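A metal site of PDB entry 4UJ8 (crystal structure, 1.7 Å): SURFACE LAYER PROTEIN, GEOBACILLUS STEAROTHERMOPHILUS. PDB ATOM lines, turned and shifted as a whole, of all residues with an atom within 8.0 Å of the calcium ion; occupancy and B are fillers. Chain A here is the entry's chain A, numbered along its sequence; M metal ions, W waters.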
ATOM      1  N   ILE A  22       9.155  -8.452 -13.943  1.00  0.00           N
ATOM      2  CA  ILE A  22       9.183  -7.543 -12.807  1.00  0.00           C
ATOM      3  C   ILE A  22       8.360  -6.313 -13.185  1.00  0.00           C
ATOM      4  O   ILE A  22       8.679  -5.643 -14.173  1.00  0.00           O
ATOM      5  CB  ILE A  22      10.631  -7.135 -12.452  1.00  0.00           C
ATOM      6  CG1 ILE A  22      11.464  -8.374 -12.119  1.00  0.00           C
ATOM      7  CG2 ILE A  22      10.675  -6.070 -11.344  1.00  0.00           C
ATOM      8  CD1 ILE A  22      12.952  -8.081 -11.967  1.00  0.00           C
ATOM      9  N   ASP A  23       7.299  -6.024 -12.437  1.00  0.00           N
ATOM     10  CA  ASP A  23       6.363  -4.936 -12.811  1.00  0.00           C
ATOM     11  C   ASP A  23       6.643  -3.712 -11.952  1.00  0.00           C
ATOM     12  O   ASP A  23       6.407  -3.712 -10.743  1.00  0.00           O
ATOM     13  CB  ASP A  23       4.908  -5.423 -12.652  1.00  0.00           C
ATOM     14  CG  ASP A  23       3.887  -4.445 -13.211  1.00  0.00           C
ATOM     15  OD1 ASP A  23       4.237  -3.270 -13.435  1.00  0.00           O
ATOM     16  OD2 ASP A  23       2.714  -4.855 -13.414  1.00  0.00           O
ATOM     17  N   LYS A  24       7.196  -2.669 -12.558  1.00  0.00           N
ATOM     18  CA  LYS A  24       7.659  -1.523 -11.782  1.00  0.00           C
ATOM     19  C   LYS A  24       6.505  -0.571 -11.515  1.00  0.00           C
ATOM     20  O   LYS A  24       6.718   0.525 -10.995  1.00  0.00           O
ATOM     21  CB  LYS A  24       8.813  -0.809 -12.479  1.00  0.00           C
ATOM     22  CG  LYS A  24       8.480  -0.207 -13.825  1.00  0.00           C
ATOM     23  CD  LYS A  24       9.660   0.618 -14.302  1.00  0.00           C
ATOM     24  CE  LYS A  24       9.323   1.369 -15.555  1.00  0.00           C
ATOM     25  NZ  LYS A  24      10.456   2.253 -15.991  1.00  0.00           N
ATOM     26  N   SER A  25       5.294  -0.986 -11.854  1.00  0.00           N
ATOM     27  CA  SER A  25       4.106  -0.284 -11.353  1.00  0.00           C
ATOM     28  C   SER A  25       4.127  -0.279  -9.822  1.00  0.00           C
ATOM     29  O   SER A  25       4.713  -1.157  -9.185  1.00  0.00           O
ATOM     30  CB  SER A  25       2.835  -0.929 -11.867  1.00  0.00           C
ATOM     31  OG  SER A  25       1.696  -0.488 -11.134  1.00  0.00           O
ATOM     32  N   ALA A  26       3.478   0.705  -9.214  1.00  0.00           N
ATOM     33  CA  ALA A  26       3.474   0.774  -7.762  1.00  0.00           C
ATOM     34  C   ALA A  26       2.269   0.056  -7.163  1.00  0.00           C
ATOM     35  O   ALA A  26       2.203  -0.140  -5.941  1.00  0.00           O
ATOM     36  CB  ALA A  26       3.514   2.233  -7.302  1.00  0.00           C
ATOM     37  N   THR A  27       1.341  -0.349  -8.019  1.00  0.00           N
ATOM     38  CA  THR A  27       0.074  -0.893  -7.556  1.00  0.00           C
ATOM     39  C   THR A  27      -0.438  -2.198  -8.180  1.00  0.00           C
ATOM     40  O   THR A  27      -1.577  -2.572  -7.929  1.00  0.00           O
ATOM     41  CB  THR A  27      -1.067   0.128  -7.745  1.00  0.00           C
ATOM     42  OG1 THR A  27      -1.210   0.437  -9.140  1.00  0.00           O
ATOM     43  CG2 THR A  27      -0.784   1.402  -6.962  1.00  0.00           C
ATOM     44  N   GLU A  28       0.361  -2.890  -8.991  1.00  0.00           N
ATOM     45  CA  GLU A  28      -0.178  -4.053  -9.684  1.00  0.00           C
ATOM     46  C   GLU A  28      -0.667  -5.117  -8.692  1.00  0.00           C
ATOM     47  O   GLU A  28      -0.086  -5.296  -7.615  1.00  0.00           O
ATOM     48  CB  GLU A  28       0.829  -4.672 -10.674  1.00  0.00           C
ATOM     49  CG  GLU A  28       1.913  -5.565 -10.055  1.00  0.00           C
ATOM     50  CD  GLU A  28       3.066  -4.756  -9.497  1.00  0.00           C
ATOM     51  OE1 GLU A  28       3.045  -3.510  -9.648  1.00  0.00           O
ATOM     52  OE2 GLU A  28       3.998  -5.356  -8.916  1.00  0.00           O
ATOM     53  N   SER A  29      -1.740  -5.793  -9.072  1.00  0.00           N
ATOM     54  CA  SER A  29      -2.334  -6.870  -8.267  1.00  0.00           C
ATOM     55  C   SER A  29      -2.505  -8.129  -9.118  1.00  0.00           C
ATOM     56  O   SER A  29      -3.159  -8.086 -10.156  1.00  0.00           O
ATOM     57  CB  SER A  29      -3.694  -6.424  -7.691  1.00  0.00           C
ATOM     58  OG  SER A  29      -4.376  -7.522  -7.090  1.00  0.00           O
ATOM     59  N   PRO A  30      -1.897  -9.260  -8.694  1.00  0.00           N
ATOM     60  CA  PRO A  30      -1.096  -9.349  -7.474  1.00  0.00           C
ATOM     61  C   PRO A  30       0.277  -8.694  -7.634  1.00  0.00           C
ATOM     62  O   PRO A  30       0.676  -8.398  -8.759  1.00  0.00           O
ATOM     63  CB  PRO A  30      -0.941 -10.862  -7.255  1.00  0.00           C
ATOM     64  CG  PRO A  30      -1.079 -11.450  -8.606  1.00  0.00           C
ATOM     65  CD  PRO A  30      -1.990 -10.555  -9.400  1.00  0.00           C
ATOM     66  N   ALA A  31       0.946  -8.425  -6.526  1.00  0.00           N
ATOM     67  CA  ALA A  31       2.278  -7.824  -6.579  1.00  0.00           C
ATOM     68  C   ALA A  31       3.172  -8.717  -7.425  1.00  0.00           C
ATOM     69  O   ALA A  31       3.104  -9.942  -7.330  1.00  0.00           O
ATOM     70  CB  ALA A  31       2.836  -7.653  -5.187  1.00  0.00           C
ATOM     71  N   ASN A  32       3.992  -8.085  -8.256  1.00  0.00           N
ATOM     72  CA  ASN A  32       4.834  -8.789  -9.213  1.00  0.00           C
ATOM     73  C   ASN A  32       6.214  -8.143  -9.265  1.00  0.00           C
ATOM     74  O   ASN A  32       6.598  -7.575 -10.289  1.00  0.00           O
ATOM     75  CB  ASN A  32       4.179  -8.783 -10.589  1.00  0.00           C
ATOM     76  CG  ASN A  32       4.878  -9.699 -11.574  1.00  0.00           C
ATOM     77  OD1 ASN A  32       5.750 -10.462 -11.179  1.00  0.00           O
ATOM     78  ND2 ASN A  32       4.498  -9.635 -12.852  1.00  0.00           N
ATOM     79  N   ASN A  33       6.961  -8.231  -8.164  1.00  0.00           N
ATOM     80  CA  ASN A  33       8.151  -7.406  -8.014  1.00  0.00           C
ATOM     81  C   ASN A  33       9.462  -8.167  -8.038  1.00  0.00           C
ATOM     82  O   ASN A  33      10.515  -7.624  -7.688  1.00  0.00           O
ATOM     83  CB  ASN A  33       8.051  -6.607  -6.720  1.00  0.00           C
ATOM     84  CG  ASN A  33       6.956  -5.577  -6.796  1.00  0.00           C
ATOM     85  OD1 ASN A  33       6.851  -4.859  -7.784  1.00  0.00           O
ATOM     86  ND2 ASN A  33       6.118  -5.510  -5.769  1.00  0.00           N
ATOM     87  N   ASP A  34       9.416  -9.423  -8.452  1.00  0.00           N
ATOM     88  CA  ASP A  34      10.669 -10.123  -8.612  1.00  0.00           C
ATOM     89  C   ASP A  34      10.611 -11.179  -9.689  1.00  0.00           C
ATOM     90  O   ASP A  34       9.565 -11.415 -10.293  1.00  0.00           O
ATOM     91  CB  ASP A  34      11.137 -10.762  -7.271  1.00  0.00           C
ATOM     92  CG  ASP A  34      10.196 -11.830  -6.734  1.00  0.00           C
ATOM     93  OD1 ASP A  34       9.472 -12.499  -7.500  1.00  0.00           O
ATOM     94  OD2 ASP A  34      10.206 -12.034  -5.499  1.00  0.00           O
ATOM     95  N   ASP A  87      13.864  -5.151  -9.500  1.00  0.00           N
ATOM     96  CA  ASP A  87      14.128  -3.864 -10.105  1.00  0.00           C
ATOM     97  C   ASP A  87      14.974  -3.019  -9.188  1.00  0.00           C
ATOM     98  O   ASP A  87      14.742  -2.939  -7.993  1.00  0.00           O
ATOM     99  CB  ASP A  87      12.808  -3.161 -10.423  1.00  0.00           C
ATOM    100  CG  ASP A  87      12.990  -1.808 -11.123  1.00  0.00           C
ATOM    101  OD1 ASP A  87      14.076  -1.583 -11.664  1.00  0.00           O
ATOM    102  OD2 ASP A  87      12.039  -0.977 -11.151  1.00  0.00           O
ATOM    103  N   ILE A 115       8.563  -4.746 -16.750  1.00  0.00           N
ATOM    104  CA  ILE A 115       7.370  -4.212 -17.395  1.00  0.00           C
ATOM    105  C   ILE A 115       6.791  -3.116 -16.513  1.00  0.00           C
ATOM    106  O   ILE A 115       7.281  -2.858 -15.417  1.00  0.00           O
ATOM    107  CB  ILE A 115       6.285  -5.294 -17.652  1.00  0.00           C
ATOM    108  CG1 ILE A 115       5.731  -5.828 -16.334  1.00  0.00           C
ATOM    109  CG2 ILE A 115       6.852  -6.441 -18.500  1.00  0.00           C
ATOM    110  CD1 ILE A 115       4.578  -6.816 -16.496  1.00  0.00           C
ATOM    111  N   ASP A 116       5.754  -2.463 -17.010  1.00  0.00           N
ATOM    112  CA  ASP A 116       5.089  -1.429 -16.236  1.00  0.00           C
ATOM    113  C   ASP A 116       3.624  -1.372 -16.632  1.00  0.00           C
ATOM    114  O   ASP A 116       3.293  -0.878 -17.717  1.00  0.00           O
ATOM    115  CB  ASP A 116       5.771  -0.064 -16.419  1.00  0.00           C
ATOM    116  CG  ASP A 116       5.252   0.977 -15.459  1.00  0.00           C
ATOM    117  OD1 ASP A 116       4.211   0.706 -14.822  1.00  0.00           O
ATOM    118  OD2 ASP A 116       5.871   2.053 -15.327  1.00  0.00           O
ATOM    119  N   THR A 117       2.749  -1.871 -15.777  1.00  0.00           N
ATOM    120  CA  THR A 117       1.331  -1.950 -16.124  1.00  0.00           C
ATOM    121  C   THR A 117       0.519  -0.775 -15.545  1.00  0.00           C
ATOM    122  O   THR A 117      -0.703  -0.831 -15.522  1.00  0.00           O
ATOM    123  CB  THR A 117       0.693  -3.283 -15.655  1.00  0.00           C
ATOM    124  OG1 THR A 117       0.829  -3.443 -14.232  1.00  0.00           O
ATOM    125  CG2 THR A 117       1.360  -4.454 -16.385  1.00  0.00           C
ATOM    126  N   THR A 118       1.215   0.265 -15.102  1.00  0.00           N
ATOM    127  CA  THR A 118       0.536   1.462 -14.596  1.00  0.00           C
ATOM    128  C   THR A 118      -0.509   1.962 -15.588  1.00  0.00           C
ATOM    129  O   THR A 118      -0.272   1.968 -16.805  1.00  0.00           O
ATOM    130  CB  THR A 118       1.561   2.587 -14.285  1.00  0.00           C
ATOM    131  OG1 THR A 118       2.479   2.129 -13.297  1.00  0.00           O
ATOM    132  CG2 THR A 118       0.860   3.868 -13.766  1.00  0.00           C
HETATM  133 CA    CA M   1       5.317  -3.385  -8.622  1.00  0.00          CA
HETATM  134  O   HOH W   1       7.033  -2.010  -7.678  1.00  0.00           O
HETATM  135  O   HOH W   2       4.319  -3.162  -6.500  1.00  0.00           O
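The nearest printed residue that does not touch the calcium ion is Lys 24 (4.2 Å).
The calcium ion is bound by OD1 of Asn 33 (2.3 Å), water W2 (2.4 Å), O of Ser 25 (2.4 Å), OE2 of Glu 28 (2.4 Å), water W1 (2.4 Å), O of Asp 23 (2.4 Å) and OE1 of Glu 28 (2.5 Å).
N of Ser 25 is in hydrogen-bond range of OD1 of Asp 23, 3.0 Å away. The backbone NH (N) of Thr 27 lies within hydrogen-bond range of the side-chain hydroxyl (OG) of Ser 25. The side-chain hydroxyl of Thr 118 sits close to the side-chain hydroxyl of Ser 25. The side-chain carboxylate (OE2) of Glu 28 lies close to the backbone NH (N) of Asn 32 (2.8 Å). N of Asp 23 is in hydrogen-bond range of O of Asn 32, at 2.7 Å. The side-chain carboxylate (OD2) of Asp 23 lies within hydrogen-bond range of the side-chain hydroxyl (OG1) of Thr 117 (2.5 Å).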
